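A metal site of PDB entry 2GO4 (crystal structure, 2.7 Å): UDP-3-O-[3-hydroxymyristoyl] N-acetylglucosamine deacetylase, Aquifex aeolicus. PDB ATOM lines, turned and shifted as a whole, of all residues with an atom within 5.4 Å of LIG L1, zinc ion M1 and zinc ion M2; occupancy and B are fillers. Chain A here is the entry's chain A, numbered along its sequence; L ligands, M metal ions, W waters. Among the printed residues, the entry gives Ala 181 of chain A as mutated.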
ATOM      1  N   ILE A  18      13.243  -4.056  10.708  1.00  0.00           N
ATOM      2  CA  ILE A  18      11.825  -4.306  10.932  1.00  0.00           C
ATOM      3  C   ILE A  18      11.492  -5.254  12.093  1.00  0.00           C
ATOM      4  O   ILE A  18      10.437  -5.127  12.721  1.00  0.00           O
ATOM      5  CB  ILE A  18      11.144  -4.820   9.629  1.00  0.00           C
ATOM      6  CG1 ILE A  18       9.627  -4.742   9.805  1.00  0.00           C
ATOM      7  CG2 ILE A  18      11.598  -6.261   9.302  1.00  0.00           C
ATOM      8  CD1 ILE A  18       8.847  -4.862   8.509  1.00  0.00           C
ATOM      9  N   HIS A  19      12.374  -6.186  12.407  1.00  0.00           N
ATOM     10  CA  HIS A  19      12.089  -7.110  13.490  1.00  0.00           C
ATOM     11  C   HIS A  19      12.689  -6.741  14.840  1.00  0.00           C
ATOM     12  O   HIS A  19      12.034  -6.867  15.870  1.00  0.00           O
ATOM     13  CB  HIS A  19      12.516  -8.526  13.116  1.00  0.00           C
ATOM     14  CG  HIS A  19      11.672  -9.157  12.060  1.00  0.00           C
ATOM     15  ND1 HIS A  19      10.291  -9.193  12.137  1.00  0.00           N
ATOM     16  CD2 HIS A  19      11.993  -9.802  10.915  1.00  0.00           C
ATOM     17  CE1 HIS A  19       9.809  -9.834  11.088  1.00  0.00           C
ATOM     18  NE2 HIS A  19      10.816 -10.214  10.327  1.00  0.00           N
ATOM     19  N   ASN A  57      11.453 -17.811   9.643  1.00  0.00           N
ATOM     20  CA  ASN A  57      10.111 -17.387  10.007  1.00  0.00           C
ATOM     21  C   ASN A  57      10.040 -15.867   9.949  1.00  0.00           C
ATOM     22  O   ASN A  57      10.706 -15.182  10.726  1.00  0.00           O
ATOM     23  CB  ASN A  57       9.751 -17.825  11.430  1.00  0.00           C
ATOM     24  CG  ASN A  57       9.735 -19.330  11.596  1.00  0.00           C
ATOM     25  OD1 ASN A  57       9.530 -19.823  12.700  1.00  0.00           O
ATOM     26  ND2 ASN A  57       9.949 -20.055  10.493  1.00  0.00           N
ATOM     27  N   HIS A  58       9.240 -15.339   9.030  1.00  0.00           N
ATOM     28  CA  HIS A  58       9.074 -13.891   8.901  1.00  0.00           C
ATOM     29  C   HIS A  58      10.275 -13.162   8.330  1.00  0.00           C
ATOM     30  O   HIS A  58      10.254 -11.947   8.183  1.00  0.00           O
ATOM     31  CB  HIS A  58       8.707 -13.289  10.261  1.00  0.00           C
ATOM     32  CG  HIS A  58       7.515 -13.944  10.890  1.00  0.00           C
ATOM     33  ND1 HIS A  58       6.247 -13.856  10.340  1.00  0.00           N
ATOM     34  CD2 HIS A  58       7.407 -14.736  11.978  1.00  0.00           C
ATOM     35  CE1 HIS A  58       5.414 -14.586  11.062  1.00  0.00           C
ATOM     36  NE2 HIS A  58       6.090 -15.128  12.062  1.00  0.00           N
ATOM     37  N   SER A  59      11.323 -13.911   8.016  1.00  0.00           N
ATOM     38  CA  SER A  59      12.528 -13.325   7.440  1.00  0.00           C
ATOM     39  C   SER A  59      13.544 -14.415   7.297  1.00  0.00           C
ATOM     40  O   SER A  59      13.376 -15.493   7.842  1.00  0.00           O
ATOM     41  CB  SER A  59      13.113 -12.233   8.335  1.00  0.00           C
ATOM     42  OG  SER A  59      13.753 -12.757   9.487  1.00  0.00           O
ATOM     43  N   GLU A  73      17.286 -11.127   3.029  1.00  0.00           N
ATOM     44  CA  GLU A  73      16.582 -11.313   1.761  1.00  0.00           C
ATOM     45  C   GLU A  73      16.395 -10.117   0.845  1.00  0.00           C
ATOM     46  O   GLU A  73      16.543 -10.257  -0.369  1.00  0.00           O
ATOM     47  CB  GLU A  73      15.221 -11.968   2.020  1.00  0.00           C
ATOM     48  CG  GLU A  73      14.266 -11.091   2.798  1.00  0.00           C
ATOM     49  CD  GLU A  73      14.131 -11.508   4.242  1.00  0.00           C
ATOM     50  OE1 GLU A  73      15.114 -12.039   4.810  1.00  0.00           O
ATOM     51  OE2 GLU A  73      13.034 -11.296   4.811  1.00  0.00           O
ATOM     52  N   HIS A  74      16.076  -8.951   1.361  1.00  0.00           N
ATOM     53  CA  HIS A  74      15.854  -7.824   0.475  1.00  0.00           C
ATOM     54  C   HIS A  74      17.137  -7.294  -0.196  1.00  0.00           C
ATOM     55  O   HIS A  74      17.148  -6.966  -1.379  1.00  0.00           O
ATOM     56  CB  HIS A  74      15.115  -6.710   1.205  1.00  0.00           C
ATOM     57  CG  HIS A  74      13.766  -7.135   1.707  1.00  0.00           C
ATOM     58  ND1 HIS A  74      12.915  -6.272   2.379  1.00  0.00           N
ATOM     59  CD2 HIS A  74      13.129  -8.320   1.656  1.00  0.00           C
ATOM     60  CE1 HIS A  74      11.818  -6.923   2.708  1.00  0.00           C
ATOM     61  NE2 HIS A  74      11.916  -8.166   2.287  1.00  0.00           N
ATOM     62  N   GLY A 101      10.711  -0.954   3.166  1.00  0.00           N
ATOM     63  CA  GLY A 101      10.072  -2.254   3.074  1.00  0.00           C
ATOM     64  C   GLY A 101      10.287  -2.968   1.748  1.00  0.00           C
ATOM     65  O   GLY A 101       9.985  -4.164   1.643  1.00  0.00           O
ATOM     66  N   THR A 179       7.118  -4.915   1.882  1.00  0.00           N
ATOM     67  CA  THR A 179       6.801  -5.987   2.818  1.00  0.00           C
ATOM     68  C   THR A 179       5.360  -5.765   3.269  1.00  0.00           C
ATOM     69  O   THR A 179       4.945  -4.640   3.570  1.00  0.00           O
ATOM     70  CB  THR A 179       7.702  -5.902   4.047  1.00  0.00           C
ATOM     71  OG1 THR A 179       9.054  -6.094   3.646  1.00  0.00           O
ATOM     72  CG2 THR A 179       7.312  -6.927   5.078  1.00  0.00           C
ATOM     73  N   PHE A 180       4.592  -6.841   3.355  1.00  0.00           N
ATOM     74  CA  PHE A 180       3.208  -6.694   3.772  1.00  0.00           C
ATOM     75  C   PHE A 180       2.862  -7.707   4.861  1.00  0.00           C
ATOM     76  O   PHE A 180       3.481  -8.766   4.978  1.00  0.00           O
ATOM     77  CB  PHE A 180       2.302  -6.901   2.559  1.00  0.00           C
ATOM     78  CG  PHE A 180       2.279  -8.305   2.078  1.00  0.00           C
ATOM     79  CD1 PHE A 180       1.365  -9.223   2.589  1.00  0.00           C
ATOM     80  CD2 PHE A 180       3.230  -8.743   1.151  1.00  0.00           C
ATOM     81  CE1 PHE A 180       1.387 -10.550   2.193  1.00  0.00           C
ATOM     82  CE2 PHE A 180       3.272 -10.070   0.744  1.00  0.00           C
ATOM     83  CZ  PHE A 180       2.350 -10.980   1.268  1.00  0.00           C
ATOM     84  N   ALA A 181       1.849  -7.375   5.650  1.00  0.00           N
ATOM     85  CA  ALA A 181       1.380  -8.256   6.718  1.00  0.00           C
ATOM     86  C   ALA A 181      -0.100  -7.995   6.904  1.00  0.00           C
ATOM     87  O   ALA A 181      -0.605  -6.923   6.548  1.00  0.00           O
ATOM     88  CB  ALA A 181       2.132  -7.996   8.021  1.00  0.00           C
ATOM     89  N   ASP A 183      -3.419  -7.619   9.428  1.00  0.00           N
ATOM     90  CA  ASP A 183      -3.685  -7.165  10.791  1.00  0.00           C
ATOM     91  C   ASP A 183      -3.765  -8.327  11.773  1.00  0.00           C
ATOM     92  O   ASP A 183      -3.325  -8.210  12.929  1.00  0.00           O
ATOM     93  CB  ASP A 183      -4.956  -6.304  10.861  1.00  0.00           C
ATOM     94  CG  ASP A 183      -6.129  -6.915  10.118  1.00  0.00           C
ATOM     95  OD1 ASP A 183      -6.155  -8.141   9.928  1.00  0.00           O
ATOM     96  OD2 ASP A 183      -7.047  -6.158   9.750  1.00  0.00           O
ATOM     97  N   GLU A 185      -2.094 -11.109  11.710  1.00  0.00           N
ATOM     98  CA  GLU A 185      -0.749 -11.654  11.942  1.00  0.00           C
ATOM     99  C   GLU A 185       0.004 -10.886  13.032  1.00  0.00           C
ATOM    100  O   GLU A 185       0.712 -11.476  13.859  1.00  0.00           O
ATOM    101  CB  GLU A 185       0.095 -11.538  10.677  1.00  0.00           C
ATOM    102  CG  GLU A 185      -0.116 -12.536   9.575  1.00  0.00           C
ATOM    103  CD  GLU A 185       1.021 -12.447   8.557  1.00  0.00           C
ATOM    104  OE1 GLU A 185       1.200 -11.369   7.943  1.00  0.00           O
ATOM    105  OE2 GLU A 185       1.762 -13.446   8.392  1.00  0.00           O
ATOM    106  N   ILE A 186      -0.144  -9.573  13.001  1.00  0.00           N
ATOM    107  CA  ILE A 186       0.541  -8.667  13.906  1.00  0.00           C
ATOM    108  C   ILE A 186       0.647  -9.039  15.388  1.00  0.00           C
ATOM    109  O   ILE A 186       1.744  -9.034  15.954  1.00  0.00           O
ATOM    110  CB  ILE A 186      -0.063  -7.261  13.767  1.00  0.00           C
ATOM    111  CG1 ILE A 186       0.102  -6.786  12.327  1.00  0.00           C
ATOM    112  CG2 ILE A 186       0.627  -6.285  14.722  1.00  0.00           C
ATOM    113  CD1 ILE A 186      -0.469  -5.423  12.049  1.00  0.00           C
ATOM    114  N   HIS A 188       0.526 -11.786  16.718  1.00  0.00           N
ATOM    115  CA  HIS A 188       1.372 -12.952  16.793  1.00  0.00           C
ATOM    116  C   HIS A 188       2.828 -12.588  16.602  1.00  0.00           C
ATOM    117  O   HIS A 188       3.691 -12.968  17.394  1.00  0.00           O
ATOM    118  CB  HIS A 188       0.988 -13.943  15.713  1.00  0.00           C
ATOM    119  CG  HIS A 188       2.104 -14.860  15.320  1.00  0.00           C
ATOM    120  ND1 HIS A 188       2.560 -15.862  16.140  1.00  0.00           N
ATOM    121  CD2 HIS A 188       2.864 -14.904  14.201  1.00  0.00           C
ATOM    122  CE1 HIS A 188       3.567 -16.489  15.547  1.00  0.00           C
ATOM    123  NE2 HIS A 188       3.767 -15.924  14.369  1.00  0.00           N
ATOM    124  N   ILE A 189       3.107 -11.847  15.542  1.00  0.00           N
ATOM    125  CA  ILE A 189       4.472 -11.433  15.265  1.00  0.00           C
ATOM    126  C   ILE A 189       5.032 -10.685  16.468  1.00  0.00           C
ATOM    127  O   ILE A 189       6.171 -10.902  16.857  1.00  0.00           O
ATOM    128  CB  ILE A 189       4.540 -10.543  13.998  1.00  0.00           C
ATOM    129  CG1 ILE A 189       4.228 -11.405  12.771  1.00  0.00           C
ATOM    130  CG2 ILE A 189       5.911  -9.915  13.863  1.00  0.00           C
ATOM    131  CD1 ILE A 189       4.090 -10.618  11.502  1.00  0.00           C
ATOM    132  N   LYS A 190       4.212  -9.811  17.052  1.00  0.00           N
ATOM    133  CA  LYS A 190       4.659  -9.058  18.230  1.00  0.00           C
ATOM    134  C   LYS A 190       4.931  -9.983  19.415  1.00  0.00           C
ATOM    135  O   LYS A 190       5.892  -9.781  20.165  1.00  0.00           O
ATOM    136  CB  LYS A 190       3.619  -8.007  18.598  1.00  0.00           C
ATOM    137  CG  LYS A 190       3.622  -6.777  17.704  1.00  0.00           C
ATOM    138  CD  LYS A 190       4.851  -5.932  17.973  1.00  0.00           C
ATOM    139  CE  LYS A 190       4.768  -4.593  17.264  1.00  0.00           C
ATOM    140  NZ  LYS A 190       5.849  -3.677  17.738  1.00  0.00           N
ATOM    141  N   VAL A 192       5.924 -13.210  19.451  1.00  0.00           N
ATOM    142  CA  VAL A 192       7.130 -14.017  19.278  1.00  0.00           C
ATOM    143  C   VAL A 192       8.429 -13.212  19.207  1.00  0.00           C
ATOM    144  O   VAL A 192       9.468 -13.745  18.826  1.00  0.00           O
ATOM    145  CB  VAL A 192       7.023 -14.892  18.011  1.00  0.00           C
ATOM    146  CG1 VAL A 192       5.819 -15.809  18.133  1.00  0.00           C
ATOM    147  CG2 VAL A 192       6.888 -14.015  16.770  1.00  0.00           C
ATOM    148  N   LEU A 194       9.043 -10.382  17.309  1.00  0.00           N
ATOM    149  CA  LEU A 194       9.402  -9.808  16.020  1.00  0.00           C
ATOM    150  C   LEU A 194       8.661  -8.511  15.738  1.00  0.00           C
ATOM    151  O   LEU A 194       8.023  -7.952  16.620  1.00  0.00           O
ATOM    152  CB  LEU A 194       9.147 -10.846  14.926  1.00  0.00           C
ATOM    153  CG  LEU A 194       9.892 -12.172  15.144  1.00  0.00           C
ATOM    154  CD1 LEU A 194       9.580 -13.132  14.018  1.00  0.00           C
ATOM    155  CD2 LEU A 194      11.388 -11.909  15.212  1.00  0.00           C
ATOM    156  N   GLY A 195       8.787  -8.026  14.507  1.00  0.00           N
ATOM    157  CA  GLY A 195       8.118  -6.805  14.094  1.00  0.00           C
ATOM    158  C   GLY A 195       8.282  -5.595  15.000  1.00  0.00           C
ATOM    159  O   GLY A 195       7.501  -4.643  14.895  1.00  0.00           O
ATOM    160  N   GLY A 198       8.407  -2.442  12.972  1.00  0.00           N
ATOM    161  CA  GLY A 198       7.447  -2.272  11.888  1.00  0.00           C
ATOM    162  C   GLY A 198       6.433  -1.166  12.060  1.00  0.00           C
ATOM    163  O   GLY A 198       5.838  -0.982  13.110  1.00  0.00           O
ATOM    164  N   SER A 199       6.216  -0.420  10.986  1.00  0.00           N
ATOM    165  CA  SER A 199       5.245   0.672  11.000  1.00  0.00           C
ATOM    166  C   SER A 199       4.576   0.716   9.642  1.00  0.00           C
ATOM    167  O   SER A 199       4.817  -0.153   8.802  1.00  0.00           O
ATOM    168  CB  SER A 199       5.953   1.993  11.282  1.00  0.00           C
ATOM    169  OG  SER A 199       6.821   2.331  10.219  1.00  0.00           O
ATOM    170  N   LEU A 200       3.728   1.706   9.418  1.00  0.00           N
ATOM    171  CA  LEU A 200       3.072   1.816   8.133  1.00  0.00           C
ATOM    172  C   LEU A 200       4.045   2.451   7.147  1.00  0.00           C
ATOM    173  O   LEU A 200       3.736   2.602   5.966  1.00  0.00           O
ATOM    174  CB  LEU A 200       1.807   2.673   8.239  1.00  0.00           C
ATOM    175  CG  LEU A 200       0.674   2.109   9.105  1.00  0.00           C
ATOM    176  CD1 LEU A 200      -0.544   3.016   8.954  1.00  0.00           C
ATOM    177  CD2 LEU A 200       0.319   0.695   8.687  1.00  0.00           C
ATOM    178  N   THR A 203       5.927  -1.168   6.168  1.00  0.00           N
ATOM    179  CA  THR A 203       5.091  -2.355   6.007  1.00  0.00           C
ATOM    180  C   THR A 203       3.730  -1.968   5.446  1.00  0.00           C
ATOM    181  O   THR A 203       3.183  -0.918   5.763  1.00  0.00           O
ATOM    182  CB  THR A 203       4.864  -3.061   7.376  1.00  0.00           C
ATOM    183  OG1 THR A 203       6.132  -3.283   8.022  1.00  0.00           O
ATOM    184  CG2 THR A 203       4.149  -4.402   7.172  1.00  0.00           C
ATOM    185  N   VAL A 205       0.060  -2.876   5.646  1.00  0.00           N
ATOM    186  CA  VAL A 205      -0.869  -3.661   6.454  1.00  0.00           C
ATOM    187  C   VAL A 205      -2.210  -3.818   5.780  1.00  0.00           C
ATOM    188  O   VAL A 205      -2.837  -2.851   5.334  1.00  0.00           O
ATOM    189  CB  VAL A 205      -1.052  -3.049   7.864  1.00  0.00           C
ATOM    190  CG1 VAL A 205      -1.744  -4.061   8.776  1.00  0.00           C
ATOM    191  CG2 VAL A 205       0.303  -2.639   8.437  1.00  0.00           C
ATOM    192  N   TYR A 212      -4.734  -0.530   5.452  1.00  0.00           N
ATOM    193  CA  TYR A 212      -4.474   0.479   6.469  1.00  0.00           C
ATOM    194  C   TYR A 212      -3.624   1.623   5.981  1.00  0.00           C
ATOM    195  O   TYR A 212      -3.893   2.767   6.326  1.00  0.00           O
ATOM    196  CB  TYR A 212      -3.811  -0.155   7.690  1.00  0.00           C
ATOM    197  CG  TYR A 212      -4.724  -1.067   8.452  1.00  0.00           C
ATOM    198  CD1 TYR A 212      -4.974  -2.364   8.013  1.00  0.00           C
ATOM    199  CD2 TYR A 212      -5.341  -0.641   9.632  1.00  0.00           C
ATOM    200  CE1 TYR A 212      -5.818  -3.213   8.713  1.00  0.00           C
ATOM    201  CE2 TYR A 212      -6.186  -1.489  10.346  1.00  0.00           C
ATOM    202  CZ  TYR A 212      -6.415  -2.763   9.881  1.00  0.00           C
ATOM    203  OH  TYR A 212      -7.228  -3.616  10.580  1.00  0.00           O
ATOM    204  N   HIS A 226       6.020  -8.836  -4.186  1.00  0.00           N
ATOM    205  CA  HIS A 226       7.002  -8.848  -3.108  1.00  0.00           C
ATOM    206  C   HIS A 226       7.436 -10.262  -2.787  1.00  0.00           C
ATOM    207  O   HIS A 226       8.579 -10.504  -2.426  1.00  0.00           O
ATOM    208  CB  HIS A 226       6.458  -8.194  -1.848  1.00  0.00           C
ATOM    209  CG  HIS A 226       7.481  -8.081  -0.759  1.00  0.00           C
ATOM    210  ND1 HIS A 226       8.442  -7.093  -0.748  1.00  0.00           N
ATOM    211  CD2 HIS A 226       7.753  -8.889   0.289  1.00  0.00           C
ATOM    212  CE1 HIS A 226       9.268  -7.303   0.258  1.00  0.00           C
ATOM    213  NE2 HIS A 226       8.873  -8.377   0.910  1.00  0.00           N
ATOM    214  N   LYS A 227       6.510 -11.202  -2.907  1.00  0.00           N
ATOM    215  CA  LYS A 227       6.844 -12.594  -2.652  1.00  0.00           C
ATOM    216  C   LYS A 227       7.843 -13.075  -3.700  1.00  0.00           C
ATOM    217  O   LYS A 227       8.702 -13.904  -3.412  1.00  0.00           O
ATOM    218  CB  LYS A 227       5.581 -13.433  -2.662  1.00  0.00           C
ATOM    219  CG  LYS A 227       4.766 -13.301  -1.403  1.00  0.00           C
ATOM    220  CD  LYS A 227       5.404 -14.070  -0.263  1.00  0.00           C
ATOM    221  CE  LYS A 227       4.733 -13.760   1.060  1.00  0.00           C
ATOM    222  NZ  LYS A 227       5.296 -14.610   2.146  1.00  0.00           N
ATOM    223  N   PHE A 229       9.989 -11.044  -5.204  1.00  0.00           N
ATOM    224  CA  PHE A 229      11.182 -10.347  -4.760  1.00  0.00           C
ATOM    225  C   PHE A 229      11.854 -11.141  -3.615  1.00  0.00           C
ATOM    226  O   PHE A 229      13.072 -11.302  -3.608  1.00  0.00           O
ATOM    227  CB  PHE A 229      10.788  -8.955  -4.266  1.00  0.00           C
ATOM    228  CG  PHE A 229      11.935  -8.126  -3.773  1.00  0.00           C
ATOM    229  CD1 PHE A 229      12.834  -7.530  -4.670  1.00  0.00           C
ATOM    230  CD2 PHE A 229      12.111  -7.897  -2.417  1.00  0.00           C
ATOM    231  CE1 PHE A 229      13.879  -6.724  -4.207  1.00  0.00           C
ATOM    232  CE2 PHE A 229      13.154  -7.091  -1.941  1.00  0.00           C
ATOM    233  CZ  PHE A 229      14.048  -6.498  -2.845  1.00  0.00           C
ATOM    234  N   ASP A 230      11.064 -11.633  -2.659  1.00  0.00           N
ATOM    235  CA  ASP A 230      11.650 -12.393  -1.556  1.00  0.00           C
ATOM    236  C   ASP A 230      12.290 -13.679  -2.049  1.00  0.00           C
ATOM    237  O   ASP A 230      13.373 -14.025  -1.610  1.00  0.00           O
ATOM    238  CB  ASP A 230      10.610 -12.785  -0.491  1.00  0.00           C
ATOM    239  CG  ASP A 230      10.248 -11.648   0.448  1.00  0.00           C
ATOM    240  OD1 ASP A 230      11.078 -10.738   0.654  1.00  0.00           O
ATOM    241  OD2 ASP A 230       9.137 -11.688   1.004  1.00  0.00           O
ATOM    242  N   HIS A 253       9.744 -18.121   2.972  1.00  0.00           N
ATOM    243  CA  HIS A 253      11.167 -18.295   3.233  1.00  0.00           C
ATOM    244  C   HIS A 253      11.558 -19.737   3.569  1.00  0.00           C
ATOM    245  O   HIS A 253      12.489 -20.281   2.977  1.00  0.00           O
ATOM    246  CB  HIS A 253      11.614 -17.354   4.352  1.00  0.00           C
ATOM    247  CG  HIS A 253      11.455 -15.913   4.031  1.00  0.00           C
ATOM    248  ND1 HIS A 253      12.090 -15.309   2.956  1.00  0.00           N
ATOM    249  CD2 HIS A 253      10.761 -14.927   4.647  1.00  0.00           C
ATOM    250  CE1 HIS A 253      11.788 -14.026   2.930  1.00  0.00           C
ATOM    251  NE2 HIS A 253      10.979 -13.761   3.938  1.00  0.00           N
HETATM  252  C1  LIG L   1       6.378 -11.184   7.079  1.00  0.00           C
HETATM  253  C2  LIG L   1       5.179 -12.123   6.980  1.00  0.00           C
HETATM  254  C3  LIG L   1       5.663 -13.551   6.694  1.00  0.00           C
HETATM  255  C4  LIG L   1       7.198 -11.268   5.791  1.00  0.00           C
HETATM  256  C5  LIG L   1       7.575 -12.731   5.510  1.00  0.00           C
HETATM  257  O1  LIG L   1       6.389 -13.547   5.455  1.00  0.00           O
HETATM  258  O2  LIG L   1       5.923  -9.835   7.249  1.00  0.00           O
HETATM  259  O3  LIG L   1       7.078  -9.872   9.192  1.00  0.00           O
HETATM  260  C6  LIG L   1       6.385  -9.246   8.389  1.00  0.00           C
HETATM  261  C7  LIG L   1       5.975  -7.794   8.658  1.00  0.00           C
HETATM  262  C8  LIG L   1       6.265  -7.358  10.094  1.00  0.00           C
HETATM  263  C9  LIG L   1       5.235  -6.295  10.514  1.00  0.00           C
HETATM  264  C10 LIG L   1       5.536  -5.712  11.893  1.00  0.00           C
HETATM  265  C11 LIG L   1       4.304  -5.084  12.544  1.00  0.00           C
HETATM  266  C12 LIG L   1       3.647  -3.977  11.712  1.00  0.00           C
HETATM  267  C13 LIG L   1       2.546  -3.313  12.534  1.00  0.00           C
HETATM  268  C14 LIG L   1       1.755  -2.281  11.732  1.00  0.00           C
HETATM  269  C15 LIG L   1       0.810  -1.500  12.655  1.00  0.00           C
HETATM  270  C16 LIG L   1      -0.077  -0.515  11.896  1.00  0.00           C
HETATM  271  C17 LIG L   1      -1.301  -1.173  11.246  1.00  0.00           C
HETATM  272  C18 LIG L   1      -2.434  -1.478  12.245  1.00  0.00           C
HETATM  273  C19 LIG L   1      -2.071  -2.583  13.239  1.00  0.00           C
HETATM  274  C20 LIG L   1       8.440 -10.383   5.905  1.00  0.00           C
HETATM  275  C21 LIG L   1       9.141 -10.166   4.559  1.00  0.00           C
HETATM  276  O4  LIG L   1       8.752  -9.296   3.779  1.00  0.00           O
HETATM  277  N1  LIG L   1      10.164 -10.983   4.321  1.00  0.00           N
HETATM  278  O5  LIG L   1      10.874 -10.834   3.171  1.00  0.00           O
HETATM  279  O6  LIG L   1       4.460 -12.099   8.213  1.00  0.00           O
HETATM  280  C22 LIG L   1       4.462 -14.490   6.609  1.00  0.00           C
HETATM  281  O7  LIG L   1       4.901 -15.842   6.501  1.00  0.00           O
HETATM  282 CL1  LG2 L   2       4.949 -18.030  12.246  1.00  0.00          CL
HETATM  283 ZN    ZN M   1      10.210  -9.350   2.083  1.00  0.00          ZN
HETATM  284 ZN    ZN M   2       5.755 -16.710  13.503  1.00  0.00          ZN
HETATM  285  O   HOH W   1       7.520 -17.359  14.775  1.00  0.00           O
HETATM  286  O   HOH W   2       7.894 -16.279   6.153  1.00  0.00           O
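Zinc ion M1 is bound by an oxygen (O5) of LIG L1 (2.0 Å), a ring nitrogen (NE2) of His 226 (2.0 Å), a ring nitrogen (NE2) of His 74 (2.1 Å), the side-chain carboxylate of Asp 230 (2.2 Å) and an oxygen (O4) of LIG L1 (2.2 Å).
Slightly farther from zinc ion M1 lies the side-chain carboxylate (OD2) of Asp 230 (2.8 Å).
The nearest printed residue that does not touch zinc ion M2 is Val 192 (4.4 Å).
The side-chain carboxylate (OE2) of Glu 73 lies within hydrogen-bond range of a ring nitrogen (NE2) of His 253.
The side-chain hydroxyl (OG1) of Thr 179 is in hydrogen-bond range of the backbone carbonyl oxygen (O) of Gly 101, at 2.9 Å.
ND1 of His 19 is in hydrogen-bond range of N of Gly 195.
O of Val 205 lies within hydrogen-bond range of N of Tyr 212, at 3.0 Å.
NZ of Lys 190 lies within hydrogen-bond range of O of Gly 195 (3.4 Å).
The backbone carbonyl oxygen (O) of Ile 189 lies within hydrogen-bond range of the backbone NH (N) of Leu 194 (3.0 Å).
N of Gly 198 is in hydrogen-bond range of O of Ile 18, 3.4 Å away.
The side-chain hydroxyl of Tyr 212 sits at hydrogen-bond distance from the side-chain carboxylate of Asp 183 (2.7 Å).
Water W2 lies within hydrogen-bond range of O7 of LIG L1 (3.0 Å) and N of His 58 (3.3 Å).
Zinc ion M2 is bound by CL1 of LG2 L2 (2.0 Å), NE2 of His 58 (2.2 Å), water W1 (2.3 Å) and NE2 of His 188 (2.3 Å).
Zinc ion M2 has four donor atoms within binding distance.
Residues that only touch zinc ion M1: Thr 179 (3.8 Å).
The nearest printed residue that does not touch zinc ion M1 is Glu 73 (4.4 Å).
Ile 18 touches LIG L1.
CE1 of His 19 touches O3 of LIG L1, at 3.3 Å.
Phe 180 touches LIG L1.
Ala 181 touches LIG L1.
Ile 186 touches LIG L1 (CD1 to C19, 3.5 Å).
Ile 189 touches LIG L1 (CD1 to O6, 3.6 Å).
Gly 195 touches LIG L1.
Gly 198 touches LIG L1 (CA to C10, 3.9 Å).
Leu 200 touches LIG L1.
Thr 203 touches LIG L1 (CG2 to C9, 3.99 Å).
CG2 of Val 205 touches C17 of LIG L1 (3.6 Å).
Tyr 212 touches LIG L1.
Lys 227 touches LIG L1 (NZ to O1, 3.6 Å).
Hydrophobic or aromatic side chains that line LIG L1: Ile 18, His 19, His 58, His 74, Ala 181, Ile 186, Ile 189, Leu 200, Val 205, Tyr 212, His 226 and His 253.
Of the 31 residues printed, 21 come within 4 Å of LIG L1.
The nearest printed residue that does not touch LIG L1 is Ser 199 (4.4 Å).
A ring nitrogen (ND1) of His 58 is in hydrogen-bond range of an oxygen (O6) of LIG L1 (3.3 Å).
The side-chain carboxylate of Glu 73 is in hydrogen-bond range of a nitrogen (N1) of LIG L1 (2.9 Å).
NE2 of His 253 lies within hydrogen-bond range of N1 of LIG L1, 2.9 Å away.
An oxygen (O6) of LIG L1 sits at hydrogen-bond distance from the side-chain carboxylate (OE2) of Glu 185.
An oxygen (O4) of LIG L1 sits close to the side-chain hydroxyl of Thr 179 (3.2 Å).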
